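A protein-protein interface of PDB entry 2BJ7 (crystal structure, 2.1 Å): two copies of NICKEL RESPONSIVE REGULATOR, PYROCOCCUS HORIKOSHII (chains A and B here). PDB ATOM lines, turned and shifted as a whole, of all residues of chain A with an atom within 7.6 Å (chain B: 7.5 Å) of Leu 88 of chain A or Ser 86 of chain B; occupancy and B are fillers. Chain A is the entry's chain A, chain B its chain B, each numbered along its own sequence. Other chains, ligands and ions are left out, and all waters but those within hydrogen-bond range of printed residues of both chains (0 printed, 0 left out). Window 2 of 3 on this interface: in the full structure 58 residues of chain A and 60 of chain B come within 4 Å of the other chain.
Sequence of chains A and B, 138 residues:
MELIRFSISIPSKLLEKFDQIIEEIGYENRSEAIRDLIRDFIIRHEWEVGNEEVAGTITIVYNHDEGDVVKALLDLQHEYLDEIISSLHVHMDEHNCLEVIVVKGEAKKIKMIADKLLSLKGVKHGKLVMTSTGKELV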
ATOM      1  N   ILE A  58       2.908   7.313  31.433  1.00  0.00           N
ATOM      2  CA  ILE A  58       1.842   8.263  31.602  1.00  0.00           C
ATOM      3  C   ILE A  58       1.026   8.144  30.328  1.00  0.00           C
ATOM      4  O   ILE A  58       1.508   8.443  29.232  1.00  0.00           O
ATOM      5  CB  ILE A  58       2.399   9.686  31.750  1.00  0.00           C
ATOM      6  CG1 ILE A  58       3.377   9.728  32.929  1.00  0.00           C
ATOM      7  CG2 ILE A  58       1.260  10.671  31.951  1.00  0.00           C
ATOM      8  CD1 ILE A  58       4.216  10.982  32.991  1.00  0.00           C
ATOM      9  N   ILE A  60      -2.211   9.288  28.115  1.00  0.00           N
ATOM     10  CA  ILE A  60      -3.120  10.418  27.989  1.00  0.00           C
ATOM     11  C   ILE A  60      -3.855  10.393  26.667  1.00  0.00           C
ATOM     12  O   ILE A  60      -3.352   9.885  25.668  1.00  0.00           O
ATOM     13  CB  ILE A  60      -2.387  11.781  28.096  1.00  0.00           C
ATOM     14  CG1 ILE A  60      -1.347  11.901  26.989  1.00  0.00           C
ATOM     15  CG2 ILE A  60      -1.737  11.921  29.460  1.00  0.00           C
ATOM     16  CD1 ILE A  60      -0.749  13.275  26.859  1.00  0.00           C
ATOM     17  N   TYR A  62      -6.339  13.005  24.162  1.00  0.00           N
ATOM     18  CA  TYR A  62      -6.765  14.380  23.943  1.00  0.00           C
ATOM     19  C   TYR A  62      -7.119  14.652  22.493  1.00  0.00           C
ATOM     20  O   TYR A  62      -6.795  13.866  21.594  1.00  0.00           O
ATOM     21  CB  TYR A  62      -5.648  15.335  24.366  1.00  0.00           C
ATOM     22  CG  TYR A  62      -4.333  15.057  23.667  1.00  0.00           C
ATOM     23  CD1 TYR A  62      -4.051  15.597  22.410  1.00  0.00           C
ATOM     24  CD2 TYR A  62      -3.381  14.228  24.251  1.00  0.00           C
ATOM     25  CE1 TYR A  62      -2.844  15.314  21.757  1.00  0.00           C
ATOM     26  CE2 TYR A  62      -2.180  13.936  23.609  1.00  0.00           C
ATOM     27  CZ  TYR A  62      -1.917  14.479  22.368  1.00  0.00           C
ATOM     28  OH  TYR A  62      -0.729  14.165  21.743  1.00  0.00           O
ATOM     29  N   GLN A  77       7.141  18.567  28.232  1.00  0.00           N
ATOM     30  CA  GLN A  77       7.993  17.388  28.131  1.00  0.00           C
ATOM     31  C   GLN A  77       9.438  17.746  27.843  1.00  0.00           C
ATOM     32  O   GLN A  77      10.362  17.125  28.376  1.00  0.00           O
ATOM     33  CB  GLN A  77       7.479  16.441  27.042  1.00  0.00           C
ATOM     34  CG  GLN A  77       6.138  15.814  27.377  1.00  0.00           C
ATOM     35  CD  GLN A  77       5.716  14.778  26.362  1.00  0.00           C
ATOM     36  OE1 GLN A  77       6.439  13.818  26.102  1.00  0.00           O
ATOM     37  NE2 GLN A  77       4.538  14.963  25.785  1.00  0.00           N
ATOM     38  N   SER A  86      10.871   8.418  26.040  1.00  0.00           N
ATOM     39  CA  SER A  86      10.249   8.446  24.721  1.00  0.00           C
ATOM     40  C   SER A  86       8.746   8.468  24.913  1.00  0.00           C
ATOM     41  O   SER A  86       8.255   8.265  26.025  1.00  0.00           O
ATOM     42  CB  SER A  86      10.603   7.182  23.925  1.00  0.00           C
ATOM     43  OG  SER A  86      12.000   7.062  23.745  1.00  0.00           O
ATOM     44  N   SER A  87       8.021   8.712  23.828  1.00  0.00           N
ATOM     45  CA  SER A  87       6.563   8.716  23.873  1.00  0.00           C
ATOM     46  C   SER A  87       6.027   8.028  22.627  1.00  0.00           C
ATOM     47  O   SER A  87       6.565   8.199  21.528  1.00  0.00           O
ATOM     48  CB  SER A  87       6.018  10.142  23.943  1.00  0.00           C
ATOM     49  OG  SER A  87       6.318  10.867  22.774  1.00  0.00           O
ATOM     50  N   LEU A  88       4.973   7.238  22.817  1.00  0.00           N
ATOM     51  CA  LEU A  88       4.322   6.513  21.733  1.00  0.00           C
ATOM     52  C   LEU A  88       3.000   7.221  21.469  1.00  0.00           C
ATOM     53  O   LEU A  88       2.259   7.537  22.396  1.00  0.00           O
ATOM     54  CB  LEU A  88       4.083   5.067  22.152  1.00  0.00           C
ATOM     55  CG  LEU A  88       3.340   4.114  21.207  1.00  0.00           C
ATOM     56  CD1 LEU A  88       4.074   4.005  19.892  1.00  0.00           C
ATOM     57  CD2 LEU A  88       3.238   2.742  21.865  1.00  0.00           C
ATOM     58  N   HIS A  89       2.711   7.477  20.200  1.00  0.00           N
ATOM     59  CA  HIS A  89       1.495   8.181  19.824  1.00  0.00           C
ATOM     60  C   HIS A  89       0.665   7.348  18.849  1.00  0.00           C
ATOM     61  O   HIS A  89       1.200   6.766  17.904  1.00  0.00           O
ATOM     62  CB  HIS A  89       1.868   9.524  19.185  1.00  0.00           C
ATOM     63  CG  HIS A  89       0.696  10.373  18.799  1.00  0.00           C
ATOM     64  ND1 HIS A  89       0.519  11.654  19.278  1.00  0.00           N
ATOM     65  CD2 HIS A  89      -0.334  10.144  17.948  1.00  0.00           C
ATOM     66  CE1 HIS A  89      -0.566  12.179  18.737  1.00  0.00           C
ATOM     67  NE2 HIS A  89      -1.102  11.284  17.924  1.00  0.00           N
ATOM     68  N   VAL A  90      -0.636   7.276  19.106  1.00  0.00           N
ATOM     69  CA  VAL A  90      -1.555   6.555  18.231  1.00  0.00           C
ATOM     70  C   VAL A  90      -2.683   7.515  17.845  1.00  0.00           C
ATOM     71  O   VAL A  90      -3.313   8.126  18.712  1.00  0.00           O
ATOM     72  CB  VAL A  90      -2.169   5.318  18.927  1.00  0.00           C
ATOM     73  CG1 VAL A  90      -3.191   4.656  17.996  1.00  0.00           C
ATOM     74  CG2 VAL A  90      -1.066   4.314  19.287  1.00  0.00           C
ATOM     75  N   CYS A  97      -6.106  11.718  19.896  1.00  0.00           N
ATOM     76  CA  CYS A  97      -4.816  11.052  19.980  1.00  0.00           C
ATOM     77  C   CYS A  97      -4.629  10.413  21.350  1.00  0.00           C
ATOM     78  O   CYS A  97      -5.093  10.938  22.364  1.00  0.00           O
ATOM     79  CB  CYS A  97      -3.674  12.060  19.784  1.00  0.00           C
ATOM     80  SG  CYS A  97      -3.684  13.030  18.248  1.00  0.00           S
ATOM     81  N   LEU A  98      -3.948   9.272  21.370  1.00  0.00           N
ATOM     82  CA  LEU A  98      -3.629   8.604  22.615  1.00  0.00           C
ATOM     83  C   LEU A  98      -2.113   8.662  22.635  1.00  0.00           C
ATOM     84  O   LEU A  98      -1.464   8.408  21.621  1.00  0.00           O
ATOM     85  CB  LEU A  98      -4.105   7.148  22.619  1.00  0.00           C
ATOM     86  CG  LEU A  98      -3.794   6.400  23.929  1.00  0.00           C
ATOM     87  CD1 LEU A  98      -4.844   5.348  24.179  1.00  0.00           C
ATOM     88  CD2 LEU A  98      -2.411   5.780  23.868  1.00  0.00           C
ATOM     89  N   GLU A  99      -1.543   9.009  23.777  1.00  0.00           N
ATOM     90  CA  GLU A  99      -0.100   9.102  23.887  1.00  0.00           C
ATOM     91  C   GLU A  99       0.343   8.408  25.169  1.00  0.00           C
ATOM     92  O   GLU A  99      -0.349   8.469  26.189  1.00  0.00           O
ATOM     93  CB  GLU A  99       0.304  10.583  23.909  1.00  0.00           C
ATOM     94  CG  GLU A  99       1.792  10.875  23.761  1.00  0.00           C
ATOM     95  CD  GLU A  99       2.096  12.381  23.730  1.00  0.00           C
ATOM     96  OE1 GLU A  99       1.334  13.139  23.089  1.00  0.00           O
ATOM     97  OE2 GLU A  99       3.107  12.810  24.335  1.00  0.00           O
ATOM     98  N   VAL A 100       1.476   7.717  25.111  1.00  0.00           N
ATOM     99  CA  VAL A 100       2.019   7.060  26.290  1.00  0.00           C
ATOM    100  C   VAL A 100       3.451   7.541  26.428  1.00  0.00           C
ATOM    101  O   VAL A 100       4.266   7.350  25.530  1.00  0.00           O
ATOM    102  CB  VAL A 100       2.042   5.531  26.167  1.00  0.00           C
ATOM    103  CG1 VAL A 100       2.502   4.927  27.486  1.00  0.00           C
ATOM    104  CG2 VAL A 100       0.683   5.018  25.803  1.00  0.00           C
ATOM    105  N   ILE A 101       3.746   8.173  27.556  1.00  0.00           N
ATOM    106  CA  ILE A 101       5.074   8.706  27.828  1.00  0.00           C
ATOM    107  C   ILE A 101       5.794   7.818  28.829  1.00  0.00           C
ATOM    108  O   ILE A 101       5.286   7.579  29.927  1.00  0.00           O
ATOM    109  CB  ILE A 101       4.960  10.119  28.402  1.00  0.00           C
ATOM    110  CG1 ILE A 101       4.138  10.987  27.447  1.00  0.00           C
ATOM    111  CG2 ILE A 101       6.338  10.709  28.627  1.00  0.00           C
ATOM    112  CD1 ILE A 101       3.718  12.321  28.028  1.00  0.00           C
ATOM    113  N   VAL A 102       6.959   7.305  28.445  1.00  0.00           N
ATOM    114  CA  VAL A 102       7.740   6.460  29.342  1.00  0.00           C
ATOM    115  C   VAL A 102       8.724   7.336  30.111  1.00  0.00           C
ATOM    116  O   VAL A 102       9.447   8.147  29.524  1.00  0.00           O
ATOM    117  CB  VAL A 102       8.517   5.380  28.578  1.00  0.00           C
ATOM    118  CG1 VAL A 102       9.336   4.551  29.558  1.00  0.00           C
ATOM    119  CG2 VAL A 102       7.556   4.489  27.819  1.00  0.00           C
ATOM    120  N   GLY B  56      -6.674   1.332  25.893  1.00  0.00           N
ATOM    121  CA  GLY B  56      -5.929   1.210  27.126  1.00  0.00           C
ATOM    122  C   GLY B  56      -4.474   0.908  26.873  1.00  0.00           C
ATOM    123  O   GLY B  56      -4.034   0.776  25.726  1.00  0.00           O
ATOM    124  N   THR B  57      -3.718   0.822  27.956  1.00  0.00           N
ATOM    125  CA  THR B  57      -2.305   0.504  27.879  1.00  0.00           C
ATOM    126  C   THR B  57      -2.005  -0.480  28.984  1.00  0.00           C
ATOM    127  O   THR B  57      -2.623  -0.458  30.054  1.00  0.00           O
ATOM    128  CB  THR B  57      -1.400   1.755  28.051  1.00  0.00           C
ATOM    129  OG1 THR B  57      -1.686   2.402  29.298  1.00  0.00           O
ATOM    130  CG2 THR B  57      -1.633   2.732  26.908  1.00  0.00           C
ATOM    131  N   GLN B  77       0.668 -11.811  22.684  1.00  0.00           N
ATOM    132  CA  GLN B  77       0.399 -10.610  21.899  1.00  0.00           C
ATOM    133  C   GLN B  77       0.035 -10.906  20.449  1.00  0.00           C
ATOM    134  O   GLN B  77      -0.898 -10.314  19.899  1.00  0.00           O
ATOM    135  CB  GLN B  77       1.597  -9.656  21.954  1.00  0.00           C
ATOM    136  CG  GLN B  77       1.886  -9.133  23.358  1.00  0.00           C
ATOM    137  CD  GLN B  77       2.858  -7.967  23.369  1.00  0.00           C
ATOM    138  OE1 GLN B  77       2.635  -6.945  22.713  1.00  0.00           O
ATOM    139  NE2 GLN B  77       3.943  -8.112  24.122  1.00  0.00           N
ATOM    140  N   LEU B  81      -3.792  -9.765  17.470  1.00  0.00           N
ATOM    141  CA  LEU B  81      -3.373  -8.775  16.481  1.00  0.00           C
ATOM    142  C   LEU B  81      -4.369  -7.653  16.257  1.00  0.00           C
ATOM    143  O   LEU B  81      -3.979  -6.525  15.967  1.00  0.00           O
ATOM    144  CB  LEU B  81      -3.108  -9.451  15.135  1.00  0.00           C
ATOM    145  CG  LEU B  81      -2.042 -10.541  15.134  1.00  0.00           C
ATOM    146  CD1 LEU B  81      -1.910 -11.116  13.736  1.00  0.00           C
ATOM    147  CD2 LEU B  81      -0.721  -9.956  15.604  1.00  0.00           C
ATOM    148  N   GLU B  83      -6.537  -6.333  18.502  1.00  0.00           N
ATOM    149  CA  GLU B  83      -6.650  -5.401  19.619  1.00  0.00           C
ATOM    150  C   GLU B  83      -5.369  -4.640  19.932  1.00  0.00           C
ATOM    151  O   GLU B  83      -5.415  -3.475  20.321  1.00  0.00           O
ATOM    152  CB  GLU B  83      -7.123  -6.127  20.885  1.00  0.00           C
ATOM    153  CG  GLU B  83      -8.551  -6.648  20.802  1.00  0.00           C
ATOM    154  CD  GLU B  83      -8.688  -7.872  19.913  1.00  0.00           C
ATOM    155  OE1 GLU B  83      -9.807  -8.116  19.416  1.00  0.00           O
ATOM    156  OE2 GLU B  83      -7.687  -8.597  19.722  1.00  0.00           O
ATOM    157  N   ILE B  84      -4.228  -5.297  19.781  1.00  0.00           N
ATOM    158  CA  ILE B  84      -2.961  -4.649  20.075  1.00  0.00           C
ATOM    159  C   ILE B  84      -2.467  -3.821  18.890  1.00  0.00           C
ATOM    160  O   ILE B  84      -2.284  -4.331  17.787  1.00  0.00           O
ATOM    161  CB  ILE B  84      -1.905  -5.683  20.469  1.00  0.00           C
ATOM    162  CG1 ILE B  84      -2.346  -6.381  21.763  1.00  0.00           C
ATOM    163  CG2 ILE B  84      -0.540  -5.000  20.631  1.00  0.00           C
ATOM    164  CD1 ILE B  84      -1.377  -7.444  22.266  1.00  0.00           C
ATOM    165  N   ILE B  85      -2.265  -2.532  19.128  1.00  0.00           N
ATOM    166  CA  ILE B  85      -1.810  -1.627  18.080  1.00  0.00           C
ATOM    167  C   ILE B  85      -0.293  -1.667  17.930  1.00  0.00           C
ATOM    168  O   ILE B  85       0.224  -1.855  16.832  1.00  0.00           O
ATOM    169  CB  ILE B  85      -2.270  -0.185  18.376  1.00  0.00           C
ATOM    170  CG1 ILE B  85      -3.801  -0.130  18.364  1.00  0.00           C
ATOM    171  CG2 ILE B  85      -1.711   0.777  17.331  1.00  0.00           C
ATOM    172  CD1 ILE B  85      -4.364   1.242  18.643  1.00  0.00           C
ATOM    173  N   SER B  86       0.417  -1.508  19.039  1.00  0.00           N
ATOM    174  CA  SER B  86       1.870  -1.525  19.013  1.00  0.00           C
ATOM    175  C   SER B  86       2.378  -1.478  20.443  1.00  0.00           C
ATOM    176  O   SER B  86       1.603  -1.264  21.379  1.00  0.00           O
ATOM    177  CB  SER B  86       2.400  -0.307  18.245  1.00  0.00           C
ATOM    178  OG  SER B  86       2.072   0.881  18.939  1.00  0.00           O
ATOM    179  N   SER B  87       3.679  -1.676  20.614  1.00  0.00           N
ATOM    180  CA  SER B  87       4.271  -1.644  21.941  1.00  0.00           C
ATOM    181  C   SER B  87       5.600  -0.897  21.946  1.00  0.00           C
ATOM    182  O   SER B  87       6.349  -0.918  20.965  1.00  0.00           O
ATOM    183  CB  SER B  87       4.469  -3.064  22.467  1.00  0.00           C
ATOM    184  OG  SER B  87       5.260  -3.826  21.584  1.00  0.00           O
ATOM    185  N   LEU B  88       5.870  -0.224  23.058  1.00  0.00           N
ATOM    186  CA  LEU B  88       7.096   0.541  23.244  1.00  0.00           C
ATOM    187  C   LEU B  88       7.919  -0.209  24.290  1.00  0.00           C
ATOM    188  O   LEU B  88       7.406  -0.569  25.355  1.00  0.00           O
ATOM    189  CB  LEU B  88       6.753   1.954  23.720  1.00  0.00           C
ATOM    190  CG  LEU B  88       7.890   2.954  23.957  1.00  0.00           C
ATOM    191  CD1 LEU B  88       8.793   3.040  22.737  1.00  0.00           C
ATOM    192  CD2 LEU B  88       7.290   4.317  24.258  1.00  0.00           C
ATOM    193  N   HIS B  89       9.188  -0.456  23.976  1.00  0.00           N
ATOM    194  CA  HIS B  89      10.074  -1.196  24.867  1.00  0.00           C
ATOM    195  C   HIS B  89      11.296  -0.368  25.236  1.00  0.00           C
ATOM    196  O   HIS B  89      11.918   0.247  24.378  1.00  0.00           O
ATOM    197  CB  HIS B  89      10.499  -2.503  24.184  1.00  0.00           C
ATOM    198  CG  HIS B  89      11.429  -3.352  24.993  1.00  0.00           C
ATOM    199  ND1 HIS B  89      11.246  -4.711  25.145  1.00  0.00           N
ATOM    200  CD2 HIS B  89      12.574  -3.052  25.652  1.00  0.00           C
ATOM    201  CE1 HIS B  89      12.237  -5.209  25.863  1.00  0.00           C
ATOM    202  NE2 HIS B  89      13.056  -4.223  26.183  1.00  0.00           N
ATOM    203  N   GLU B  99       8.015  -2.546  29.241  1.00  0.00           N
ATOM    204  CA  GLU B  99       7.258  -2.576  28.001  1.00  0.00           C
ATOM    205  C   GLU B  99       5.849  -2.050  28.210  1.00  0.00           C
ATOM    206  O   GLU B  99       5.206  -2.369  29.212  1.00  0.00           O
ATOM    207  CB  GLU B  99       7.189  -4.010  27.460  1.00  0.00           C
ATOM    208  CG  GLU B  99       6.616  -4.117  26.052  1.00  0.00           C
ATOM    209  CD  GLU B  99       6.563  -5.552  25.535  1.00  0.00           C
ATOM    210  OE1 GLU B  99       7.464  -6.352  25.872  1.00  0.00           O
ATOM    211  OE2 GLU B  99       5.626  -5.878  24.773  1.00  0.00           O
ATOM    212  N   VAL B 100       5.370  -1.232  27.278  1.00  0.00           N
ATOM    213  CA  VAL B 100       4.011  -0.727  27.380  1.00  0.00           C
ATOM    214  C   VAL B 100       3.274  -1.033  26.074  1.00  0.00           C
ATOM    215  O   VAL B 100       3.692  -0.634  24.987  1.00  0.00           O
ATOM    216  CB  VAL B 100       3.980   0.789  27.725  1.00  0.00           C
ATOM    217  CG1 VAL B 100       4.818   1.582  26.749  1.00  0.00           C
ATOM    218  CG2 VAL B 100       2.538   1.279  27.740  1.00  0.00           C
ATOM    219  N   ILE B 101       2.179  -1.773  26.201  1.00  0.00           N
ATOM    220  CA  ILE B 101       1.372  -2.204  25.063  1.00  0.00           C
ATOM    221  C   ILE B 101       0.101  -1.365  24.901  1.00  0.00           C
ATOM    222  O   ILE B 101      -0.674  -1.214  25.850  1.00  0.00           O
ATOM    223  CB  ILE B 101       0.990  -3.688  25.253  1.00  0.00           C
ATOM    224  CG1 ILE B 101       2.251  -4.499  25.570  1.00  0.00           C
ATOM    225  CG2 ILE B 101       0.304  -4.221  24.020  1.00  0.00           C
ATOM    226  CD1 ILE B 101       1.997  -5.926  25.982  1.00  0.00           C
ATOM    227  N   VAL B 102      -0.116  -0.818  23.706  1.00  0.00           N
ATOM    228  CA  VAL B 102      -1.314  -0.019  23.460  1.00  0.00           C
ATOM    229  C   VAL B 102      -2.394  -0.907  22.841  1.00  0.00           C
ATOM    230  O   VAL B 102      -2.158  -1.606  21.855  1.00  0.00           O
ATOM    231  CB  VAL B 102      -1.033   1.193  22.522  1.00  0.00           C
ATOM    232  CG1 VAL B 102      -2.322   1.951  22.258  1.00  0.00           C
ATOM    233  CG2 VAL B 102      -0.028   2.143  23.171  1.00  0.00           C
ATOM    234  N   VAL B 103      -3.583  -0.878  23.430  1.00  0.00           N
ATOM    235  CA  VAL B 103      -4.679  -1.705  22.950  1.00  0.00           C
ATOM    236  C   VAL B 103      -5.934  -0.899  22.681  1.00  0.00           C
ATOM    237  O   VAL B 103      -6.198   0.110  23.339  1.00  0.00           O
ATOM    238  CB  VAL B 103      -5.016  -2.818  23.966  1.00  0.00           C
ATOM    239  CG1 VAL B 103      -3.817  -3.730  24.150  1.00  0.00           C
ATOM    240  CG2 VAL B 103      -5.404  -2.198  25.306  1.00  0.00           C
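Of the 15 printed residues of chain A, 4 touch a printed residue of chain B. Hydrophobic or aromatic side chains of chain A that line the printed part of chain B: Leu 88, Val 90, Val 100 and Val 102. Along chain A the printed residues that touch a printed residue of chain B span positions 88 to 102. Of the 16 printed residues of chain B, 6 touch a printed residue of chain A. Hydrophobic or aromatic side chains of chain B that line the printed part of chain A: Ile 85, Leu 88, Val 100 and Val 102. Among the printed residues, 9 pairs touch across the chains. Among the printed residues, no Asp or Glu carboxylate lies within 4 Å of a Lys or Arg side-chain nitrogen of the other chain.
Of chain B, only Ser 86 (3.7 Å), Leu 88 (3.9 Å) and Val 102 (3.6 Å) come within 4 Å of Leu 88 of chain A. Of the printed residues of chain A, Val 102 of chain B touches Leu 88 (3.6 Å), Val 90 (3.999 Å) and Val 100 (3.96 Å). Printed residues of chain A within 4 Å of Leu 88 of chain B: Leu 88 (3.9 Å) and Val 102 (3.6 Å). Cys 97 of chain A touches none of the printed residues of chain B. The nearest residue of chain B that does not touch Leu 88 of chain A is Ser 87 of chain B (4.3 Å). The nearest residue of chain A that does not touch Ser 86 of chain B is Val 90 of chain A (4.7 Å).
O of Leu 88 of chain B lies within hydrogen-bond range of N of Val 100 of chain B, at 2.9 Å. The backbone carbonyl oxygen of Ser 86 of chain B sits at hydrogen-bond distance from the backbone NH of Val 102 of chain B (2.9 Å). N of Ile 85 of chain B sits at hydrogen-bond distance from O of Val 102 of chain B (2.9 Å). The backbone NH (N) of Val 90 of chain A is in hydrogen-bond range of the backbone carbonyl oxygen (O) of Leu 98 of chain A, at 2.9 Å. O of Ser 86 of chain A is in hydrogen-bond range of N of Val 102 of chain A (2.9 Å). N of Leu 88 of chain A lies within hydrogen-bond range of O of Val 100 of chain A, at 2.8 Å.
Leu 88 of chain A touches Ser 86 of chain B, but with the chains exchanged Ser 86 of chain A does not touch Leu 88 of chain B (4.4 Å). Leu 88 of chain B touches its own counterpart, Leu 88 of chain A. Leu 88 of chain A touches Val 102 of chain B, and with the chains exchanged Val 102 of chain A touches Leu 88 of chain B. Val 100 of chain A touches Val 102 of chain B, but with the chains exchanged Val 102 of chain A does not touch Val 100 of chain B (4.1 Å). Of the 9 pairs that touch across the chains among the printed residues, 4 have their exchanged pair printed and touching as well.
Ser 86 of chain B touches Leu 88 of chain A. Leu 88 of chain A touches Leu 88 of chain B (CB to CD2, 3.9 Å). Leu 88 of chain A touches Val 102 of chain B (CD2 to CG2, 3.6 Å). Ile 85 of chain B touches Val 90 of chain A (CD1 to CG1, 3.7 Å). Val 102 of chain B touches Val 90 of chain A. Thr 57 of chain B touches Val 100 of chain A. Val 100 of chain B touches Val 100 of chain A (CG2 to CG1, 3.7 Å). CG2 of Val 100 of chain A touches CG2 of Val 102 of chain B, 3.96 Å away. Leu 88 of chain B touches Val 102 of chain A.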
